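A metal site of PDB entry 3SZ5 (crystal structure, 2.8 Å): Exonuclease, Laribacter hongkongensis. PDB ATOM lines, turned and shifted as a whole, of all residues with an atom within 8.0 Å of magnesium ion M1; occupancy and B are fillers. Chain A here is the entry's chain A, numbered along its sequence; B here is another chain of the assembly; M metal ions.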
ATOM      1  N   SER A  19      -5.897  -1.955   6.603  1.00  0.00           N
ATOM      2  CA  SER A  19      -4.801  -2.655   5.920  1.00  0.00           C
ATOM      3  C   SER A  19      -5.260  -3.936   5.214  1.00  0.00           C
ATOM      4  O   SER A  19      -4.476  -4.587   4.541  1.00  0.00           O
ATOM      5  CB  SER A  19      -3.636  -2.940   6.881  1.00  0.00           C
ATOM      6  OG  SER A  19      -4.037  -3.798   7.913  1.00  0.00           O
ATOM      7  N   GLY A  64      10.292  -3.700   9.360  1.00  0.00           N
ATOM      8  CA  GLY A  64       9.230  -2.712   9.216  1.00  0.00           C
ATOM      9  C   GLY A  64       8.683  -2.238  10.551  1.00  0.00           C
ATOM     10  O   GLY A  64       8.241  -1.084  10.706  1.00  0.00           O
ATOM     11  N   GLU A  68       9.950   1.553  12.288  1.00  0.00           N
ATOM     12  CA  GLU A  68       8.816   2.455  12.168  1.00  0.00           C
ATOM     13  C   GLU A  68       9.024   3.790  12.942  1.00  0.00           C
ATOM     14  O   GLU A  68       8.914   4.877  12.354  1.00  0.00           O
ATOM     15  CB  GLU A  68       7.554   1.733  12.633  1.00  0.00           C
ATOM     16  CG  GLU A  68       6.319   2.121  11.875  1.00  0.00           C
ATOM     17  CD  GLU A  68       5.055   1.797  12.648  1.00  0.00           C
ATOM     18  OE1 GLU A  68       4.334   0.840  12.243  1.00  0.00           O
ATOM     19  OE2 GLU A  68       4.820   2.496  13.654  1.00  0.00           O
ATOM     20  N   ARG A  72       9.071   7.712  11.726  1.00  0.00           N
ATOM     21  CA  ARG A  72       8.207   8.743  12.333  1.00  0.00           C
ATOM     22  C   ARG A  72       9.071   9.964  12.661  1.00  0.00           C
ATOM     23  O   ARG A  72       8.779  11.070  12.196  1.00  0.00           O
ATOM     24  CB  ARG A  72       7.457   8.226  13.564  1.00  0.00           C
ATOM     25  CG  ARG A  72       6.188   9.017  13.954  1.00  0.00           C
ATOM     26  CD  ARG A  72       5.420   8.340  15.125  1.00  0.00           C
ATOM     27  NE  ARG A  72       4.592   7.243  14.624  1.00  0.00           N
ATOM     28  CZ  ARG A  72       4.937   5.948  14.604  1.00  0.00           C
ATOM     29  NH1 ARG A  72       6.103   5.534  15.094  1.00  0.00           N
ATOM     30  NH2 ARG A  72       4.108   5.055  14.096  1.00  0.00           N
ATOM     31  N   SER A 100      -6.078   1.885  11.817  1.00  0.00           N
ATOM     32  CA  SER A 100      -4.972   2.155  12.714  1.00  0.00           C
ATOM     33  C   SER A 100      -3.929   2.941  11.945  1.00  0.00           C
ATOM     34  O   SER A 100      -2.951   2.333  11.478  1.00  0.00           O
ATOM     35  CB  SER A 100      -4.345   0.859  13.201  1.00  0.00           C
ATOM     36  OG  SER A 100      -4.943   0.410  14.403  1.00  0.00           O
ATOM     37  N   PRO A 101      -4.114   4.279  11.799  1.00  0.00           N
ATOM     38  CA  PRO A 101      -3.090   5.037  11.071  1.00  0.00           C
ATOM     39  C   PRO A 101      -1.823   5.086  11.898  1.00  0.00           C
ATOM     40  O   PRO A 101      -1.873   4.911  13.112  1.00  0.00           O
ATOM     41  CB  PRO A 101      -3.709   6.426  10.917  1.00  0.00           C
ATOM     42  CG  PRO A 101      -4.730   6.522  11.977  1.00  0.00           C
ATOM     43  CD  PRO A 101      -5.148   5.161  12.386  1.00  0.00           C
ATOM     44  N   ASP A 102      -0.689   5.307  11.232  1.00  0.00           N
ATOM     45  CA  ASP A 102       0.605   5.365  11.911  1.00  0.00           C
ATOM     46  C   ASP A 102       0.765   6.733  12.577  1.00  0.00           C
ATOM     47  O   ASP A 102       1.712   6.940  13.329  1.00  0.00           O
ATOM     48  CB  ASP A 102       1.765   5.100  10.947  1.00  0.00           C
ATOM     49  CG  ASP A 102       1.790   3.675  10.447  1.00  0.00           C
ATOM     50  OD1 ASP A 102       1.439   2.780  11.219  1.00  0.00           O
ATOM     51  OD2 ASP A 102       2.166   3.451   9.289  1.00  0.00           O
ATOM     52  N   ILE A 111      -0.302  10.112   8.825  1.00  0.00           N
ATOM     53  CA  ILE A 111       0.862   9.455   8.232  1.00  0.00           C
ATOM     54  C   ILE A 111       0.694   7.914   8.192  1.00  0.00           C
ATOM     55  O   ILE A 111       0.242   7.287   9.175  1.00  0.00           O
ATOM     56  CB  ILE A 111       2.168   9.882   8.911  1.00  0.00           C
ATOM     57  CG1 ILE A 111       3.357   9.251   8.194  1.00  0.00           C
ATOM     58  CG2 ILE A 111       2.194   9.502  10.375  1.00  0.00           C
ATOM     59  CD1 ILE A 111       4.651   9.416   8.920  1.00  0.00           C
ATOM     60  N   GLU A 112       0.986   7.321   7.026  1.00  0.00           N
ATOM     61  CA  GLU A 112       1.112   5.878   6.888  1.00  0.00           C
ATOM     62  C   GLU A 112       2.538   5.627   6.451  1.00  0.00           C
ATOM     63  O   GLU A 112       2.990   6.222   5.479  1.00  0.00           O
ATOM     64  CB  GLU A 112       0.137   5.317   5.855  1.00  0.00           C
ATOM     65  CG  GLU A 112       0.274   3.818   5.577  1.00  0.00           C
ATOM     66  CD  GLU A 112       0.212   2.943   6.855  1.00  0.00           C
ATOM     67  OE1 GLU A 112      -0.533   3.277   7.817  1.00  0.00           O
ATOM     68  OE2 GLU A 112       0.928   1.917   6.901  1.00  0.00           O
ATOM     69  N   ILE A 113       3.227   4.753   7.203  1.00  0.00           N
ATOM     70  CA  ILE A 113       4.666   4.471   7.104  1.00  0.00           C
ATOM     71  C   ILE A 113       4.935   3.048   6.595  1.00  0.00           C
ATOM     72  O   ILE A 113       4.343   2.079   7.073  1.00  0.00           O
ATOM     73  CB  ILE A 113       5.340   4.540   8.512  1.00  0.00           C
ATOM     74  CG1 ILE A 113       5.629   5.973   8.937  1.00  0.00           C
ATOM     75  CG2 ILE A 113       6.670   3.780   8.539  1.00  0.00           C
ATOM     76  CD1 ILE A 113       5.734   6.180  10.470  1.00  0.00           C
ATOM     77  N   LYS A 114       5.841   2.923   5.635  1.00  0.00           N
ATOM     78  CA  LYS A 114       6.341   1.597   5.248  1.00  0.00           C
ATOM     79  C   LYS A 114       7.837   1.634   5.427  1.00  0.00           C
ATOM     80  O   LYS A 114       8.472   2.647   5.196  1.00  0.00           O
ATOM     81  CB  LYS A 114       6.016   1.236   3.776  1.00  0.00           C
ATOM     82  CG  LYS A 114       4.555   1.341   3.337  1.00  0.00           C
ATOM     83  CD  LYS A 114       3.602   0.780   4.366  1.00  0.00           C
ATOM     84  CE  LYS A 114       2.185   0.926   3.895  1.00  0.00           C
ATOM     85  NZ  LYS A 114       1.220   0.234   4.772  1.00  0.00           N
ATOM     86  N   CYS A 115       8.382   0.511   5.868  1.00  0.00           N
ATOM     87  CA  CYS A 115       9.816   0.323   5.962  1.00  0.00           C
ATOM     88  C   CYS A 115      10.099  -1.040   5.369  1.00  0.00           C
ATOM     89  O   CYS A 115      10.372  -1.971   6.102  1.00  0.00           O
ATOM     90  CB  CYS A 115      10.252   0.347   7.420  1.00  0.00           C
ATOM     91  SG  CYS A 115      10.030   1.925   8.208  1.00  0.00           S
ATOM     92  N   TYR A 134      -2.221   0.229  -0.925  1.00  0.00           N
ATOM     93  CA  TYR A 134      -1.964   1.212   0.099  1.00  0.00           C
ATOM     94  C   TYR A 134      -2.814   2.465  -0.100  1.00  0.00           C
ATOM     95  O   TYR A 134      -3.211   3.132   0.862  1.00  0.00           O
ATOM     96  CB  TYR A 134      -0.484   1.555   0.145  1.00  0.00           C
ATOM     97  CG  TYR A 134       0.363   0.368   0.503  1.00  0.00           C
ATOM     98  CD1 TYR A 134      -0.057  -0.565   1.443  1.00  0.00           C
ATOM     99  CD2 TYR A 134       1.601   0.173  -0.108  1.00  0.00           C
ATOM    100  CE1 TYR A 134       0.730  -1.657   1.766  1.00  0.00           C
ATOM    101  CE2 TYR A 134       2.409  -0.915   0.215  1.00  0.00           C
ATOM    102  CZ  TYR A 134       1.973  -1.830   1.151  1.00  0.00           C
ATOM    103  OH  TYR A 134       2.775  -2.908   1.466  1.00  0.00           O
ATOM    104  N   GLN A 137      -5.677   1.379   1.616  1.00  0.00           N
ATOM    105  CA  GLN A 137      -5.434   1.477   3.036  1.00  0.00           C
ATOM    106  C   GLN A 137      -5.640   2.904   3.513  1.00  0.00           C
ATOM    107  O   GLN A 137      -6.347   3.139   4.511  1.00  0.00           O
ATOM    108  CB  GLN A 137      -4.024   1.057   3.373  1.00  0.00           C
ATOM    109  CG  GLN A 137      -3.861   0.861   4.850  1.00  0.00           C
ATOM    110  CD  GLN A 137      -2.436   0.590   5.260  1.00  0.00           C
ATOM    111  OE1 GLN A 137      -1.527   0.515   4.422  1.00  0.00           O
ATOM    112  NE2 GLN A 137      -2.241   0.407   6.554  1.00  0.00           N
ATOM    113  N   GLN A 141      -8.345   4.922   6.042  1.00  0.00           N
ATOM    114  CA  GLN A 141      -7.964   5.634   7.247  1.00  0.00           C
ATOM    115  C   GLN A 141      -8.653   6.984   7.259  1.00  0.00           C
ATOM    116  O   GLN A 141      -9.164   7.433   8.286  1.00  0.00           O
ATOM    117  CB  GLN A 141      -6.452   5.809   7.286  1.00  0.00           C
ATOM    118  CG  GLN A 141      -5.688   4.526   7.550  1.00  0.00           C
ATOM    119  CD  GLN A 141      -4.218   4.659   7.208  1.00  0.00           C
ATOM    120  OE1 GLN A 141      -3.358   4.078   7.857  1.00  0.00           O
ATOM    121  NE2 GLN A 141      -3.924   5.448   6.182  1.00  0.00           N
ATOM    122  N   PHE A 152       2.184   9.602   2.702  1.00  0.00           N
ATOM    123  CA  PHE A 152       2.721   8.276   2.598  1.00  0.00           C
ATOM    124  C   PHE A 152       4.218   8.343   2.676  1.00  0.00           C
ATOM    125  O   PHE A 152       4.836   8.965   1.824  1.00  0.00           O
ATOM    126  CB  PHE A 152       2.317   7.663   1.272  1.00  0.00           C
ATOM    127  CG  PHE A 152       2.850   6.287   1.047  1.00  0.00           C
ATOM    128  CD1 PHE A 152       4.013   6.092   0.305  1.00  0.00           C
ATOM    129  CD2 PHE A 152       2.207   5.183   1.570  1.00  0.00           C
ATOM    130  CE1 PHE A 152       4.518   4.802   0.083  1.00  0.00           C
ATOM    131  CE2 PHE A 152       2.694   3.890   1.357  1.00  0.00           C
ATOM    132  CZ  PHE A 152       3.856   3.705   0.616  1.00  0.00           C
ATOM    133  N   VAL A 153       4.792   7.681   3.678  1.00  0.00           N
ATOM    134  CA  VAL A 153       6.241   7.663   3.923  1.00  0.00           C
ATOM    135  C   VAL A 153       6.835   6.276   3.700  1.00  0.00           C
ATOM    136  O   VAL A 153       6.382   5.279   4.288  1.00  0.00           O
ATOM    137  CB  VAL A 153       6.565   8.148   5.375  1.00  0.00           C
ATOM    138  CG1 VAL A 153       8.067   7.964   5.749  1.00  0.00           C
ATOM    139  CG2 VAL A 153       6.092   9.601   5.550  1.00  0.00           C
ATOM    140  OP3  DT B   1      -5.742  -0.354   9.725  1.00  0.00           O
ATOM    141  P    DT B   1      -5.453  -1.715  10.512  1.00  0.00           P
ATOM    142  OP1  DT B   1      -5.666  -2.843   9.586  1.00  0.00           O
ATOM    143  OP2  DT B   1      -6.081  -1.662  11.846  1.00  0.00           O
ATOM    144  O5'  DT B   1      -3.899  -1.577  10.808  1.00  0.00           O
ATOM    145  C5'  DT B   1      -3.247  -2.430  11.701  1.00  0.00           C
ATOM    146  C4'  DT B   1      -1.761  -2.119  11.654  1.00  0.00           C
ATOM    147  O4'  DT B   1      -1.054  -3.004  12.554  1.00  0.00           O
ATOM    148  C3'  DT B   1      -1.088  -2.304  10.284  1.00  0.00           C
ATOM    149  O3'  DT B   1       0.028  -1.427  10.283  1.00  0.00           O
ATOM    150  C2'  DT B   1      -0.697  -3.781  10.328  1.00  0.00           C
ATOM    151  C1'  DT B   1      -0.253  -3.888  11.791  1.00  0.00           C
ATOM    152  N1   DT B   1      -0.391  -5.232  12.408  1.00  0.00           N
ATOM    153  C2   DT B   1       0.618  -5.666  13.265  1.00  0.00           C
ATOM    154  O2   DT B   1       1.627  -5.015  13.525  1.00  0.00           O
ATOM    155  N3   DT B   1       0.389  -6.916  13.806  1.00  0.00           N
ATOM    156  C4   DT B   1      -0.729  -7.731  13.575  1.00  0.00           C
ATOM    157  O4   DT B   1      -0.852  -8.830  14.099  1.00  0.00           O
ATOM    158  C5   DT B   1      -1.739  -7.213  12.686  1.00  0.00           C
ATOM    159  C7   DT B   1      -2.969  -8.029  12.388  1.00  0.00           C
ATOM    160  C6   DT B   1      -1.522  -5.996  12.151  1.00  0.00           C
ATOM    161  P    DT B   2       1.099  -1.350   9.100  1.00  0.00           P
ATOM    162  OP1  DT B   2       1.773  -0.035   9.288  1.00  0.00           O
ATOM    163  OP2  DT B   2       0.428  -1.694   7.809  1.00  0.00           O
ATOM    164  O5'  DT B   2       2.137  -2.518   9.487  1.00  0.00           O
ATOM    165  C5'  DT B   2       3.281  -2.277  10.332  1.00  0.00           C
ATOM    166  C4'  DT B   2       4.314  -3.403  10.265  1.00  0.00           C
ATOM    167  O4'  DT B   2       3.860  -4.550  11.040  1.00  0.00           O
ATOM    168  C3'  DT B   2       4.643  -3.948   8.869  1.00  0.00           C
ATOM    169  O3'  DT B   2       5.774  -3.249   8.312  1.00  0.00           O
ATOM    170  C2'  DT B   2       5.006  -5.410   9.138  1.00  0.00           C
ATOM    171  C1'  DT B   2       4.206  -5.764  10.385  1.00  0.00           C
ATOM    172  N1   DT B   2       2.968  -6.592  10.090  1.00  0.00           N
ATOM    173  C2   DT B   2       2.760  -7.764  10.800  1.00  0.00           C
ATOM    174  O2   DT B   2       3.519  -8.188  11.658  1.00  0.00           O
ATOM    175  N3   DT B   2       1.622  -8.450  10.470  1.00  0.00           N
ATOM    176  C4   DT B   2       0.673  -8.098   9.515  1.00  0.00           C
ATOM    177  O4   DT B   2      -0.313  -8.813   9.321  1.00  0.00           O
ATOM    178  C5   DT B   2       0.923  -6.847   8.786  1.00  0.00           C
ATOM    179  C7   DT B   2      -0.017  -6.320   7.717  1.00  0.00           C
ATOM    180  C6   DT B   2       2.055  -6.182   9.119  1.00  0.00           C
ATOM    181  P    DT B   3       5.757  -2.563   6.859  1.00  0.00           P
ATOM    182  OP1  DT B   3       6.692  -1.415   6.905  1.00  0.00           O
ATOM    183  OP2  DT B   3       4.341  -2.375   6.477  1.00  0.00           O
ATOM    184  O5'  DT B   3       6.332  -3.707   5.869  1.00  0.00           O
ATOM    185  C5'  DT B   3       7.651  -4.275   6.003  1.00  0.00           C
ATOM    186  C4'  DT B   3       7.837  -5.390   4.994  1.00  0.00           C
ATOM    187  O4'  DT B   3       7.117  -6.570   5.442  1.00  0.00           O
ATOM    188  C3'  DT B   3       7.306  -5.088   3.576  1.00  0.00           C
ATOM    189  O3'  DT B   3       8.268  -5.462   2.552  1.00  0.00           O
ATOM    190  C2'  DT B   3       6.027  -5.906   3.525  1.00  0.00           C
ATOM    191  C1'  DT B   3       6.542  -7.125   4.280  1.00  0.00           C
ATOM    192  N1   DT B   3       5.520  -8.211   4.500  1.00  0.00           N
ATOM    193  C2   DT B   3       5.847  -9.503   4.098  1.00  0.00           C
ATOM    194  O2   DT B   3       6.926  -9.818   3.618  1.00  0.00           O
ATOM    195  N3   DT B   3       4.856 -10.440   4.304  1.00  0.00           N
ATOM    196  C4   DT B   3       3.588 -10.223   4.842  1.00  0.00           C
ATOM    197  O4   DT B   3       2.795 -11.151   4.973  1.00  0.00           O
ATOM    198  C5   DT B   3       3.314  -8.840   5.230  1.00  0.00           C
ATOM    199  C7   DT B   3       2.003  -8.422   5.836  1.00  0.00           C
ATOM    200  C6   DT B   3       4.270  -7.910   5.040  1.00  0.00           C
HETATM  201 MG    MG M   1       2.654   1.242   8.215  1.00  0.00          MG
HETATM  202 MG    MG M   2      -0.708   1.533  10.319  1.00  0.00          MG
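Merely in contact with magnesium ion M1: Lys 114. Within 4 Å of magnesium ion M1: Asp 102, Glu 112, Ile 113, Lys 114 and DT 2 of chain B. The nearest printed residue that does not touch magnesium ion M1 is DT 1 of chain B (4.3 Å).
The backbone carbonyl oxygen (O) of Glu 112 lies within hydrogen-bond range of the backbone NH (N) of Val 153 (2.9 Å). The backbone NH (N) of Lys 114 is in hydrogen-bond range of the backbone carbonyl oxygen (O) of Val 153 (2.8 Å). The side-chain carboxylate (OE2) of Glu 112 lies close to the side-chain amino group (NZ) of Lys 114, 2.7 Å away. N of Asp 102 sits at hydrogen-bond distance from O of Ile 111. The side-chain carboxylate (OE1) of Glu 112 lies close to the side-chain amide oxygen (OE1) of Gln 141, at 2.9 Å. O of Asp 102 sits at hydrogen-bond distance from NH2 of Arg 72 (3.1 Å). OP2 of DT 2 of chain B lies within salt-bridge range of the side-chain amino group of Lys 114, 3.7 Å away. NZ of Lys 114 sits at hydrogen-bond distance from OE1 of Gln 137, at 2.8 Å.
Magnesium ion M1 is bound by OP1 of DT 2 of chain B (1.9 Å), the backbone carbonyl oxygen of Ile 113 (2.2 Å), the side-chain carboxylate of Glu 112 (2.3 Å) and the side-chain carboxylate of Asp 102 (2.5 Å).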
